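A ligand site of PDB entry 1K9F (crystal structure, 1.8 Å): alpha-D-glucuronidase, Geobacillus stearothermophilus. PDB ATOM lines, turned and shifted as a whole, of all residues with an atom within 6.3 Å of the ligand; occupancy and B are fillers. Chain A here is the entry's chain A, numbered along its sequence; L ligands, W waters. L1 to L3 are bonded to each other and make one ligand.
An oxygen (O2) of LG2 L2 is in hydrogen-bond range of the side-chain carboxylate (OD2) of Asp 364 (2.5 Å).
OE2 of Glu 392 lies within hydrogen-bond range of O1 of LG3 L3, at 2.6 Å.
O5 of LG3 L3 is in salt-bridge range of NZ of Lys 359, 2.6 Å away.
NZ of Lys 281 is in salt-bridge range of O6 of LG3 L3.
An oxygen (O5) of LG3 L3 lies within salt-bridge range of the guanidinium group (NH2) of Arg 318 (2.7 Å).
An oxygen (O2) of LG3 L3 sits at hydrogen-bond distance from the side-chain carboxylate (OE2) of Glu 158.
The side-chain amide nitrogen (ND2) of Asn 201 lies close to an oxygen (O3) of LG3 L3, at 3.0 Å.
An oxygen (O3) of LG2 L2 sits at hydrogen-bond distance from the guanidinium group (NH1) of Arg 335, at 2.9 Å.
O3 of LIG L1 lies within hydrogen-bond range of NH2 of Arg 159.
NE2 of His 527 lies close to O4 of LG2 L2 (3.3 Å).
OD1 of Asp 364 lies within salt-bridge range of NZ of Lys 359, 2.7 Å away.
The side-chain carboxylate (OE2) of Glu 392 sits at hydrogen-bond distance from a ring nitrogen (ND1) of His 527 (2.7 Å).
OE1 of Glu 158 lies within hydrogen-bond range of ND2 of Asn 201 (3.1 Å).
The side-chain carboxylate (OE1) of Glu 158 is in hydrogen-bond range of the side-chain amide nitrogen (ND2) of Asn 199, 2.9 Å away.
NH2 of Arg 335 sits close to OH of Tyr 322, 3.3 Å away.
NH2 of Arg 335 is in hydrogen-bond range of O of Met 363, at 3.5 Å.
O of Gly 525 sits at hydrogen-bond distance from NH1 of Arg 159 (2.8 Å).
The side-chain hydroxyl (OH) of Tyr 393 sits close to a ring nitrogen (ND1) of His 527 (3.1 Å).
CE3 of Trp 150 touches C1 of LG3 L3, at 3.8 Å.
OD1 of Asn 199 touches C1 of LG3 L3, at 3.7 Å.
CG2 of Val 200 touches C1 of LG3 L3, 3.7 Å away.
Phe 320 touches the ligand.
OH of Tyr 322 touches C3 of LG2 L2, 3.6 Å away.
OH of Tyr 393 touches O1 of LG3 L3 (3.8 Å).
CH2 of Trp 520 touches O3 of LG2 L2 (3.5 Å).
O of Gly 525 touches O3 of LIG L1, 3.5 Å away.
OH of Tyr 535 touches O4 of LG2 L2 (3.6 Å).
Trp 540 touches the ligand.
Hydrophobic or aromatic side chains that line the ligand: Trp 150, Val 200, Phe 320, Trp 520, His 527, Tyr 535 and Trp 540.
Along chain A the residues within 4 Å of the ligand span positions 150 to 540.
Water W2 lies within hydrogen-bond range of an oxygen (O3) of LG2 L2 (2.6 Å) and the side-chain hydroxyl (OG1) of Thr 542 (2.9 Å).
Water W1 lies within hydrogen-bond range of OH of Tyr 535 (2.7 Å) and O3 of LIG L1 (3.2 Å).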
ATOM      1  N   TRP A 150       7.271   6.117 -11.158  1.00  0.00           N
ATOM      2  CA  TRP A 150       6.951   4.850 -10.509  1.00  0.00           C
ATOM      3  C   TRP A 150       7.998   3.812 -10.932  1.00  0.00           C
ATOM      4  O   TRP A 150       7.761   2.607 -10.898  1.00  0.00           O
ATOM      5  CB  TRP A 150       5.530   4.395 -10.880  1.00  0.00           C
ATOM      6  CG  TRP A 150       4.470   5.191 -10.138  1.00  0.00           C
ATOM      7  CD1 TRP A 150       4.676   6.217  -9.265  1.00  0.00           C
ATOM      8  CD2 TRP A 150       3.042   5.002 -10.193  1.00  0.00           C
ATOM      9  NE1 TRP A 150       3.473   6.688  -8.778  1.00  0.00           N
ATOM     10  CE2 TRP A 150       2.457   5.953  -9.329  1.00  0.00           C
ATOM     11  CE3 TRP A 150       2.209   4.112 -10.888  1.00  0.00           C
ATOM     12  CZ2 TRP A 150       1.073   6.047  -9.143  1.00  0.00           C
ATOM     13  CZ3 TRP A 150       0.832   4.204 -10.709  1.00  0.00           C
ATOM     14  CH2 TRP A 150       0.276   5.174  -9.847  1.00  0.00           C
ATOM     15  N   GLU A 158       6.407   0.560 -12.660  1.00  0.00           N
ATOM     16  CA  GLU A 158       5.066   0.120 -12.332  1.00  0.00           C
ATOM     17  C   GLU A 158       4.085   0.964 -13.140  1.00  0.00           C
ATOM     18  O   GLU A 158       4.120   2.197 -13.077  1.00  0.00           O
ATOM     19  CB  GLU A 158       4.798   0.258 -10.824  1.00  0.00           C
ATOM     20  CG  GLU A 158       3.460  -0.305 -10.415  1.00  0.00           C
ATOM     21  CD  GLU A 158       3.362  -0.588  -8.925  1.00  0.00           C
ATOM     22  OE1 GLU A 158       4.418  -0.630  -8.250  1.00  0.00           O
ATOM     23  OE2 GLU A 158       2.229  -0.783  -8.431  1.00  0.00           O
ATOM     24  N   ARG A 159       3.235   0.296 -13.901  1.00  0.00           N
ATOM     25  CA  ARG A 159       2.249   0.957 -14.769  1.00  0.00           C
ATOM     26  C   ARG A 159       2.988   1.785 -15.825  1.00  0.00           C
ATOM     27  O   ARG A 159       2.534   2.867 -16.205  1.00  0.00           O
ATOM     28  CB  ARG A 159       1.312   1.850 -13.953  1.00  0.00           C
ATOM     29  CG  ARG A 159       0.661   1.158 -12.765  1.00  0.00           C
ATOM     30  CD  ARG A 159      -0.015  -0.155 -13.159  1.00  0.00           C
ATOM     31  NE  ARG A 159      -0.572  -0.821 -11.975  1.00  0.00           N
ATOM     32  CZ  ARG A 159      -1.221  -1.981 -12.005  1.00  0.00           C
ATOM     33  NH1 ARG A 159      -1.402  -2.626 -13.147  1.00  0.00           N
ATOM     34  NH2 ARG A 159      -1.705  -2.488 -10.867  1.00  0.00           N
ATOM     35  N   ASN A 199       9.662   4.819  -7.523  1.00  0.00           N
ATOM     36  CA  ASN A 199       8.324   4.316  -7.235  1.00  0.00           C
ATOM     37  C   ASN A 199       7.827   4.618  -5.813  1.00  0.00           C
ATOM     38  O   ASN A 199       8.579   4.467  -4.843  1.00  0.00           O
ATOM     39  CB  ASN A 199       8.322   2.807  -7.460  1.00  0.00           C
ATOM     40  CG  ASN A 199       6.929   2.218  -7.597  1.00  0.00           C
ATOM     41  OD1 ASN A 199       5.930   2.876  -7.297  1.00  0.00           O
ATOM     42  ND2 ASN A 199       6.857   0.974  -8.038  1.00  0.00           N
ATOM     43  N   VAL A 200       6.565   5.030  -5.699  1.00  0.00           N
ATOM     44  CA  VAL A 200       5.987   5.314  -4.391  1.00  0.00           C
ATOM     45  C   VAL A 200       5.915   3.999  -3.607  1.00  0.00           C
ATOM     46  O   VAL A 200       5.851   4.007  -2.374  1.00  0.00           O
ATOM     47  CB  VAL A 200       4.599   5.956  -4.519  1.00  0.00           C
ATOM     48  CG1 VAL A 200       4.736   7.338  -5.160  1.00  0.00           C
ATOM     49  CG2 VAL A 200       3.675   5.083  -5.354  1.00  0.00           C
ATOM     50  N   ASN A 201       5.896   2.873  -4.321  1.00  0.00           N
ATOM     51  CA  ASN A 201       5.910   1.566  -3.678  1.00  0.00           C
ATOM     52  C   ASN A 201       7.411   1.280  -3.597  1.00  0.00           C
ATOM     53  O   ASN A 201       8.002   0.770  -4.558  1.00  0.00           O
ATOM     54  CB  ASN A 201       5.240   0.488  -4.531  1.00  0.00           C
ATOM     55  CG  ASN A 201       3.725   0.593  -4.518  1.00  0.00           C
ATOM     56  OD1 ASN A 201       3.119   0.824  -3.478  1.00  0.00           O
ATOM     57  ND2 ASN A 201       3.116   0.410  -5.688  1.00  0.00           N
ATOM     58  N   LYS A 281       4.006   6.934   0.728  1.00  0.00           N
ATOM     59  CA  LYS A 281       2.828   6.104   0.587  1.00  0.00           C
ATOM     60  C   LYS A 281       2.895   5.196   1.808  1.00  0.00           C
ATOM     61  O   LYS A 281       3.715   4.275   1.868  1.00  0.00           O
ATOM     62  CB  LYS A 281       2.863   5.254  -0.688  1.00  0.00           C
ATOM     63  CG  LYS A 281       1.688   4.306  -0.803  1.00  0.00           C
ATOM     64  CD  LYS A 281       1.716   3.478  -2.078  1.00  0.00           C
ATOM     65  CE  LYS A 281       0.604   2.444  -2.080  1.00  0.00           C
ATOM     66  NZ  LYS A 281       0.602   1.624  -3.331  1.00  0.00           N
ATOM     67  N   ARG A 318       0.736  11.015   0.492  1.00  0.00           N
ATOM     68  CA  ARG A 318      -0.352  10.589  -0.377  1.00  0.00           C
ATOM     69  C   ARG A 318      -1.581  10.163   0.424  1.00  0.00           C
ATOM     70  O   ARG A 318      -1.468   9.398   1.387  1.00  0.00           O
ATOM     71  CB  ARG A 318       0.111   9.437  -1.278  1.00  0.00           C
ATOM     72  CG  ARG A 318       1.214   9.838  -2.233  1.00  0.00           C
ATOM     73  CD  ARG A 318       1.601   8.685  -3.149  1.00  0.00           C
ATOM     74  NE  ARG A 318       0.681   8.502  -4.270  1.00  0.00           N
ATOM     75  CZ  ARG A 318       0.151   7.332  -4.610  1.00  0.00           C
ATOM     76  NH1 ARG A 318       0.427   6.246  -3.907  1.00  0.00           N
ATOM     77  NH2 ARG A 318      -0.638   7.239  -5.677  1.00  0.00           N
ATOM     78  N   PHE A 320      -3.986   8.420  -0.712  1.00  0.00           N
ATOM     79  CA  PHE A 320      -4.562   7.244  -1.343  1.00  0.00           C
ATOM     80  C   PHE A 320      -4.596   6.149  -0.285  1.00  0.00           C
ATOM     81  O   PHE A 320      -3.802   5.204  -0.317  1.00  0.00           O
ATOM     82  CB  PHE A 320      -3.717   6.801  -2.533  1.00  0.00           C
ATOM     83  CG  PHE A 320      -4.366   5.743  -3.383  1.00  0.00           C
ATOM     84  CD1 PHE A 320      -5.535   6.023  -4.087  1.00  0.00           C
ATOM     85  CD2 PHE A 320      -3.805   4.473  -3.501  1.00  0.00           C
ATOM     86  CE1 PHE A 320      -6.145   5.061  -4.886  1.00  0.00           C
ATOM     87  CE2 PHE A 320      -4.408   3.499  -4.303  1.00  0.00           C
ATOM     88  CZ  PHE A 320      -5.578   3.793  -4.996  1.00  0.00           C
ATOM     89  N   TYR A 322      -7.299   3.552   1.912  1.00  0.00           N
ATOM     90  CA  TYR A 322      -8.633   2.966   2.017  1.00  0.00           C
ATOM     91  C   TYR A 322      -8.508   1.516   2.469  1.00  0.00           C
ATOM     92  O   TYR A 322      -7.408   0.998   2.649  1.00  0.00           O
ATOM     93  CB  TYR A 322      -9.337   3.016   0.659  1.00  0.00           C
ATOM     94  CG  TYR A 322      -8.610   2.256  -0.423  1.00  0.00           C
ATOM     95  CD1 TYR A 322      -7.472   2.785  -1.027  1.00  0.00           C
ATOM     96  CD2 TYR A 322      -9.029   0.982  -0.817  1.00  0.00           C
ATOM     97  CE1 TYR A 322      -6.769   2.076  -2.008  1.00  0.00           C
ATOM     98  CE2 TYR A 322      -8.341   0.264  -1.797  1.00  0.00           C
ATOM     99  CZ  TYR A 322      -7.211   0.818  -2.387  1.00  0.00           C
ATOM    100  OH  TYR A 322      -6.531   0.115  -3.350  1.00  0.00           O
ATOM    101  N   ARG A 335     -15.599   2.756  -0.561  1.00  0.00           N
ATOM    102  CA  ARG A 335     -14.211   3.150  -0.745  1.00  0.00           C
ATOM    103  C   ARG A 335     -14.087   4.630  -1.121  1.00  0.00           C
ATOM    104  O   ARG A 335     -13.125   5.301  -0.734  1.00  0.00           O
ATOM    105  CB  ARG A 335     -13.551   2.271  -1.822  1.00  0.00           C
ATOM    106  CG  ARG A 335     -12.176   2.752  -2.255  1.00  0.00           C
ATOM    107  CD  ARG A 335     -11.544   1.777  -3.234  1.00  0.00           C
ATOM    108  NE  ARG A 335     -10.328   2.315  -3.825  1.00  0.00           N
ATOM    109  CZ  ARG A 335      -9.531   1.631  -4.626  1.00  0.00           C
ATOM    110  NH1 ARG A 335      -9.802   0.373  -4.936  1.00  0.00           N
ATOM    111  NH2 ARG A 335      -8.439   2.204  -5.122  1.00  0.00           N
ATOM    112  N   LYS A 359      -5.471  12.199  -5.232  1.00  0.00           N
ATOM    113  CA  LYS A 359      -5.757  11.932  -6.641  1.00  0.00           C
ATOM    114  C   LYS A 359      -6.942  12.786  -7.082  1.00  0.00           C
ATOM    115  O   LYS A 359      -7.758  13.191  -6.240  1.00  0.00           O
ATOM    116  CB  LYS A 359      -6.058  10.441  -6.858  1.00  0.00           C
ATOM    117  CG  LYS A 359      -4.860   9.540  -6.616  1.00  0.00           C
ATOM    118  CD  LYS A 359      -5.121   8.094  -6.997  1.00  0.00           C
ATOM    119  CE  LYS A 359      -3.865   7.246  -6.816  1.00  0.00           C
ATOM    120  NZ  LYS A 359      -4.066   5.845  -7.285  1.00  0.00           N
ATOM    121  N   MET A 363     -11.462   7.401  -6.149  1.00  0.00           N
ATOM    122  CA  MET A 363     -11.265   5.968  -6.360  1.00  0.00           C
ATOM    123  C   MET A 363      -9.858   5.669  -6.861  1.00  0.00           C
ATOM    124  O   MET A 363      -8.946   5.526  -6.054  1.00  0.00           O
ATOM    125  CB  MET A 363     -12.324   5.432  -7.320  1.00  0.00           C
ATOM    126  CG  MET A 363     -13.747   5.443  -6.738  1.00  0.00           C
ATOM    127  SD  MET A 363     -13.923   4.377  -5.274  1.00  0.00           S
ATOM    128  CE  MET A 363     -14.115   2.772  -6.061  1.00  0.00           C
ATOM    129  N   ASP A 364      -9.659   5.589  -8.178  1.00  0.00           N
ATOM    130  CA  ASP A 364      -8.315   5.303  -8.682  1.00  0.00           C
ATOM    131  C   ASP A 364      -8.069   5.580 -10.163  1.00  0.00           C
ATOM    132  O   ASP A 364      -8.008   4.651 -10.977  1.00  0.00           O
ATOM    133  CB  ASP A 364      -7.935   3.857  -8.354  1.00  0.00           C
ATOM    134  CG  ASP A 364      -6.519   3.494  -8.821  1.00  0.00           C
ATOM    135  OD1 ASP A 364      -5.669   4.406  -8.929  1.00  0.00           O
ATOM    136  OD2 ASP A 364      -6.271   2.289  -9.063  1.00  0.00           O
ATOM    137  N   PHE A 365      -7.946   6.852 -10.501  1.00  0.00           N
ATOM    138  CA  PHE A 365      -7.652   7.272 -11.871  1.00  0.00           C
ATOM    139  C   PHE A 365      -8.485   6.619 -12.981  1.00  0.00           C
ATOM    140  O   PHE A 365      -7.943   6.293 -14.037  1.00  0.00           O
ATOM    141  CB  PHE A 365      -6.171   7.019 -12.193  1.00  0.00           C
ATOM    142  CG  PHE A 365      -5.208   7.733 -11.286  1.00  0.00           C
ATOM    143  CD1 PHE A 365      -5.365   9.088 -11.011  1.00  0.00           C
ATOM    144  CD2 PHE A 365      -4.090   7.077 -10.783  1.00  0.00           C
ATOM    145  CE1 PHE A 365      -4.407   9.781 -10.254  1.00  0.00           C
ATOM    146  CE2 PHE A 365      -3.134   7.751 -10.021  1.00  0.00           C
ATOM    147  CZ  PHE A 365      -3.294   9.109  -9.769  1.00  0.00           C
ATOM    148  N   GLU A 386      -2.901  14.909  -7.424  1.00  0.00           N
ATOM    149  CA  GLU A 386      -2.095  13.940  -8.165  1.00  0.00           C
ATOM    150  C   GLU A 386      -2.923  13.454  -9.345  1.00  0.00           C
ATOM    151  O   GLU A 386      -4.055  13.023  -9.167  1.00  0.00           O
ATOM    152  CB  GLU A 386      -1.750  12.748  -7.270  1.00  0.00           C
ATOM    153  CG  GLU A 386      -0.852  11.698  -7.948  1.00  0.00           C
ATOM    154  CD  GLU A 386      -0.619  10.473  -7.084  1.00  0.00           C
ATOM    155  OE1 GLU A 386      -0.523  10.619  -5.844  1.00  0.00           O
ATOM    156  OE2 GLU A 386      -0.511   9.363  -7.641  1.00  0.00           O
ATOM    157  N   GLN A 388      -2.674  11.180 -13.198  1.00  0.00           N
ATOM    158  CA  GLN A 388      -1.873  10.120 -13.780  1.00  0.00           C
ATOM    159  C   GLN A 388      -1.635  10.324 -15.263  1.00  0.00           C
ATOM    160  O   GLN A 388      -2.553  10.198 -16.068  1.00  0.00           O
ATOM    161  CB  GLN A 388      -2.552   8.765 -13.512  1.00  0.00           C
ATOM    162  CG  GLN A 388      -1.667   7.559 -13.785  1.00  0.00           C
ATOM    163  CD  GLN A 388      -2.380   6.249 -13.511  1.00  0.00           C
ATOM    164  OE1 GLN A 388      -3.503   6.026 -13.962  1.00  0.00           O
ATOM    165  NE2 GLN A 388      -1.712   5.370 -12.776  1.00  0.00           N
ATOM    166  N   GLU A 392      -2.815   4.196 -17.188  1.00  0.00           N
ATOM    167  CA  GLU A 392      -3.165   2.916 -16.590  1.00  0.00           C
ATOM    168  C   GLU A 392      -4.552   2.420 -16.952  1.00  0.00           C
ATOM    169  O   GLU A 392      -4.711   1.286 -17.427  1.00  0.00           O
ATOM    170  CB  GLU A 392      -3.039   2.966 -15.061  1.00  0.00           C
ATOM    171  CG  GLU A 392      -3.398   1.644 -14.393  1.00  0.00           C
ATOM    172  CD  GLU A 392      -3.119   1.644 -12.901  1.00  0.00           C
ATOM    173  OE1 GLU A 392      -2.649   2.673 -12.372  1.00  0.00           O
ATOM    174  OE2 GLU A 392      -3.384   0.601 -12.259  1.00  0.00           O
ATOM    175  N   TYR A 393      -5.568   3.244 -16.732  1.00  0.00           N
ATOM    176  CA  TYR A 393      -6.938   2.868 -17.031  1.00  0.00           C
ATOM    177  C   TYR A 393      -7.464   3.613 -18.252  1.00  0.00           C
ATOM    178  O   TYR A 393      -8.640   3.520 -18.583  1.00  0.00           O
ATOM    179  CB  TYR A 393      -7.845   3.170 -15.835  1.00  0.00           C
ATOM    180  CG  TYR A 393      -7.445   2.445 -14.566  1.00  0.00           C
ATOM    181  CD1 TYR A 393      -7.758   1.099 -14.382  1.00  0.00           C
ATOM    182  CD2 TYR A 393      -6.795   3.127 -13.535  1.00  0.00           C
ATOM    183  CE1 TYR A 393      -7.419   0.437 -13.196  1.00  0.00           C
ATOM    184  CE2 TYR A 393      -6.455   2.475 -12.351  1.00  0.00           C
ATOM    185  CZ  TYR A 393      -6.781   1.135 -12.185  1.00  0.00           C
ATOM    186  OH  TYR A 393      -6.455   0.483 -11.003  1.00  0.00           O
ATOM    187  N   TRP A 520     -14.070   1.248 -13.824  1.00  0.00           N
ATOM    188  CA  TRP A 520     -13.565  -0.126 -13.843  1.00  0.00           C
ATOM    189  C   TRP A 520     -13.965  -0.984 -15.043  1.00  0.00           C
ATOM    190  O   TRP A 520     -13.811  -0.562 -16.176  1.00  0.00           O
ATOM    191  CB  TRP A 520     -13.918  -0.803 -12.510  1.00  0.00           C
ATOM    192  CG  TRP A 520     -13.476   0.059 -11.359  1.00  0.00           C
ATOM    193  CD1 TRP A 520     -14.205   1.042 -10.741  1.00  0.00           C
ATOM    194  CD2 TRP A 520     -12.152   0.160 -10.823  1.00  0.00           C
ATOM    195  NE1 TRP A 520     -13.410   1.737  -9.860  1.00  0.00           N
ATOM    196  CE2 TRP A 520     -12.152   1.223  -9.894  1.00  0.00           C
ATOM    197  CE3 TRP A 520     -10.955  -0.550 -11.051  1.00  0.00           C
ATOM    198  CZ2 TRP A 520     -10.997   1.600  -9.188  1.00  0.00           C
ATOM    199  CZ3 TRP A 520      -9.814  -0.173 -10.347  1.00  0.00           C
ATOM    200  CH2 TRP A 520      -9.842   0.890  -9.421  1.00  0.00           C
ATOM    201  N   PRO A 524      -8.389  -7.677 -14.189  1.00  0.00           N
ATOM    202  CA  PRO A 524      -7.661  -7.496 -12.931  1.00  0.00           C
ATOM    203  C   PRO A 524      -6.153  -7.617 -13.148  1.00  0.00           C
ATOM    204  O   PRO A 524      -5.699  -8.236 -14.114  1.00  0.00           O
ATOM    205  CB  PRO A 524      -8.195  -8.626 -12.056  1.00  0.00           C
ATOM    206  CG  PRO A 524      -9.578  -8.872 -12.600  1.00  0.00           C
ATOM    207  CD  PRO A 524      -9.350  -8.793 -14.086  1.00  0.00           C
ATOM    208  N   GLY A 525      -5.383  -7.010 -12.253  1.00  0.00           N
ATOM    209  CA  GLY A 525      -3.942  -7.089 -12.371  1.00  0.00           C
ATOM    210  C   GLY A 525      -3.314  -6.060 -13.289  1.00  0.00           C
ATOM    211  O   GLY A 525      -2.886  -5.014 -12.821  1.00  0.00           O
ATOM    212  N   HIS A 526      -3.250  -6.366 -14.584  1.00  0.00           N
ATOM    213  CA  HIS A 526      -2.649  -5.438 -15.536  1.00  0.00           C
ATOM    214  C   HIS A 526      -3.576  -4.283 -15.933  1.00  0.00           C
ATOM    215  O   HIS A 526      -3.136  -3.291 -16.498  1.00  0.00           O
ATOM    216  CB  HIS A 526      -2.166  -6.190 -16.785  1.00  0.00           C
ATOM    217  CG  HIS A 526      -3.257  -6.859 -17.556  1.00  0.00           C
ATOM    218  ND1 HIS A 526      -3.452  -8.219 -17.547  1.00  0.00           N
ATOM    219  CD2 HIS A 526      -4.193  -6.347 -18.390  1.00  0.00           C
ATOM    220  CE1 HIS A 526      -4.461  -8.524 -18.340  1.00  0.00           C
ATOM    221  NE2 HIS A 526      -4.926  -7.409 -18.863  1.00  0.00           N
ATOM    222  N   HIS A 527      -4.863  -4.434 -15.638  1.00  0.00           N
ATOM    223  CA  HIS A 527      -5.867  -3.397 -15.876  1.00  0.00           C
ATOM    224  C   HIS A 527      -6.135  -2.954 -17.309  1.00  0.00           C
ATOM    225  O   HIS A 527      -6.720  -1.894 -17.534  1.00  0.00           O
ATOM    226  CB  HIS A 527      -5.504  -2.171 -15.037  1.00  0.00           C
ATOM    227  CG  HIS A 527      -5.494  -2.442 -13.561  1.00  0.00           C
ATOM    228  ND1 HIS A 527      -4.863  -1.617 -12.654  1.00  0.00           N
ATOM    229  CD2 HIS A 527      -6.043  -3.450 -12.848  1.00  0.00           C
ATOM    230  CE1 HIS A 527      -5.021  -2.108 -11.435  1.00  0.00           C
ATOM    231  NE2 HIS A 527      -5.741  -3.218 -11.523  1.00  0.00           N
ATOM    232  N   TYR A 535     -13.337  -7.064 -11.103  1.00  0.00           N
ATOM    233  CA  TYR A 535     -13.161  -6.837  -9.672  1.00  0.00           C
ATOM    234  C   TYR A 535     -14.492  -6.788  -8.936  1.00  0.00           C
ATOM    235  O   TYR A 535     -14.541  -6.413  -7.762  1.00  0.00           O
ATOM    236  CB  TYR A 535     -12.429  -5.502  -9.448  1.00  0.00           C
ATOM    237  CG  TYR A 535     -10.936  -5.509  -9.706  1.00  0.00           C
ATOM    238  CD1 TYR A 535     -10.070  -6.271  -8.925  1.00  0.00           C
ATOM    239  CD2 TYR A 535     -10.381  -4.707 -10.708  1.00  0.00           C
ATOM    240  CE1 TYR A 535      -8.703  -6.244  -9.125  1.00  0.00           C
ATOM    241  CE2 TYR A 535      -9.006  -4.673 -10.916  1.00  0.00           C
ATOM    242  CZ  TYR A 535      -8.171  -5.440 -10.122  1.00  0.00           C
ATOM    243  OH  TYR A 535      -6.813  -5.407 -10.302  1.00  0.00           O
ATOM    244  N   TRP A 540     -11.477  -5.056  -3.290  1.00  0.00           N
ATOM    245  CA  TRP A 540     -10.977  -3.710  -3.551  1.00  0.00           C
ATOM    246  C   TRP A 540     -12.013  -2.594  -3.476  1.00  0.00           C
ATOM    247  O   TRP A 540     -11.675  -1.427  -3.665  1.00  0.00           O
ATOM    248  CB  TRP A 540     -10.273  -3.650  -4.901  1.00  0.00           C
ATOM    249  CG  TRP A 540      -9.032  -4.486  -4.977  1.00  0.00           C
ATOM    250  CD1 TRP A 540      -8.904  -5.715  -5.550  1.00  0.00           C
ATOM    251  CD2 TRP A 540      -7.736  -4.149  -4.460  1.00  0.00           C
ATOM    252  NE1 TRP A 540      -7.611  -6.166  -5.428  1.00  0.00           N
ATOM    253  CE2 TRP A 540      -6.880  -5.218  -4.767  1.00  0.00           C
ATOM    254  CE3 TRP A 540      -7.224  -3.036  -3.773  1.00  0.00           C
ATOM    255  CZ2 TRP A 540      -5.525  -5.219  -4.406  1.00  0.00           C
ATOM    256  CZ3 TRP A 540      -5.883  -3.037  -3.413  1.00  0.00           C
ATOM    257  CH2 TRP A 540      -5.040  -4.129  -3.730  1.00  0.00           C
ATOM    258  N   THR A 542     -14.463  -1.864  -5.519  1.00  0.00           N
ATOM    259  CA  THR A 542     -14.742  -1.278  -6.818  1.00  0.00           C
ATOM    260  C   THR A 542     -15.839  -2.097  -7.494  1.00  0.00           C
ATOM    261  O   THR A 542     -15.552  -2.993  -8.294  1.00  0.00           O
ATOM    262  CB  THR A 542     -13.474  -1.278  -7.685  1.00  0.00           C
ATOM    263  OG1 THR A 542     -13.011  -2.624  -7.835  1.00  0.00           O
ATOM    264  CG2 THR A 542     -12.389  -0.463  -7.024  1.00  0.00           C
HETATM  265  O1  LIG L   1       0.108  -6.108  -5.612  1.00  0.00           O
HETATM  266  C1  LIG L   1      -0.382  -5.019  -6.308  1.00  0.00           C
HETATM  267  C2  LIG L   1      -1.137  -5.489  -7.566  1.00  0.00           C
HETATM  268  C3  LIG L   1      -1.787  -4.314  -8.281  1.00  0.00           C
HETATM  269  C4  LIG L   1      -2.631  -3.514  -7.296  1.00  0.00           C
HETATM  270  C5  LIG L   1      -1.794  -3.110  -6.077  1.00  0.00           C
HETATM  271  O2  LIG L   1      -0.223  -6.130  -8.449  1.00  0.00           O
HETATM  272  O3  LIG L   1      -2.615  -4.785  -9.332  1.00  0.00           O
HETATM  273  O4  LIG L   1      -3.170  -2.339  -7.918  1.00  0.00           O
HETATM  274  O5  LIG L   1      -1.264  -4.293  -5.446  1.00  0.00           O
HETATM  275  C1  LG2 L   2      -4.434  -2.035  -7.485  1.00  0.00           C
HETATM  276  C2  LG2 L   2      -4.735  -0.537  -7.613  1.00  0.00           C
HETATM  277  C3  LG2 L   2      -6.090  -0.344  -6.891  1.00  0.00           C
HETATM  278  C4  LG2 L   2      -7.163  -1.216  -7.602  1.00  0.00           C
HETATM  279  C5  LG2 L   2      -6.723  -2.683  -7.704  1.00  0.00           C
HETATM  280  O1  LG2 L   2      -3.660   0.244  -7.003  1.00  0.00           O
HETATM  281  O2  LG2 L   2      -6.485   1.014  -6.908  1.00  0.00           O
HETATM  282  O3  LG2 L   2      -8.411  -1.143  -6.915  1.00  0.00           O
HETATM  283  O4  LG2 L   2      -5.391  -2.784  -8.255  1.00  0.00           O
HETATM  284  C1  LG3 L   3       2.238   2.466  -7.456  1.00  0.00           C
HETATM  285  C2  LG3 L   3      -3.206   1.344  -7.738  1.00  0.00           C
HETATM  286  C3  LG3 L   3      -2.261   0.975  -8.909  1.00  0.00           C
HETATM  287  C4  LG3 L   3      -0.812   0.938  -8.247  1.00  0.00           C
HETATM  288  C5  LG3 L   3      -0.273   2.087  -7.538  1.00  0.00           C
HETATM  289  C6  LG3 L   3      -1.477   2.632  -6.828  1.00  0.00           C
HETATM  290  C7  LG3 L   3      -1.217   3.797  -5.968  1.00  0.00           C
HETATM  291  O1  LG3 L   3      -2.897   0.053  -9.789  1.00  0.00           O
HETATM  292  O2  LG3 L   3      -0.095   0.516  -9.427  1.00  0.00           O
HETATM  293  O3  LG3 L   3       0.961   2.235  -6.818  1.00  0.00           O
HETATM  294  O4  LG3 L   3      -2.933   2.443  -6.887  1.00  0.00           O
HETATM  295  O5  LG3 L   3      -1.783   4.949  -6.416  1.00  0.00           O
HETATM  296  O6  LG3 L   3      -0.446   3.522  -4.878  1.00  0.00           O
HETATM  297  O   HOH W   1      -5.097  -6.635  -8.613  1.00  0.00           O
HETATM  298  O   HOH W   2     -10.093  -2.794  -8.071  1.00  0.00           O
HETATM  299  O   HOH W   3      -3.075   3.921  -9.905  1.00  0.00           O
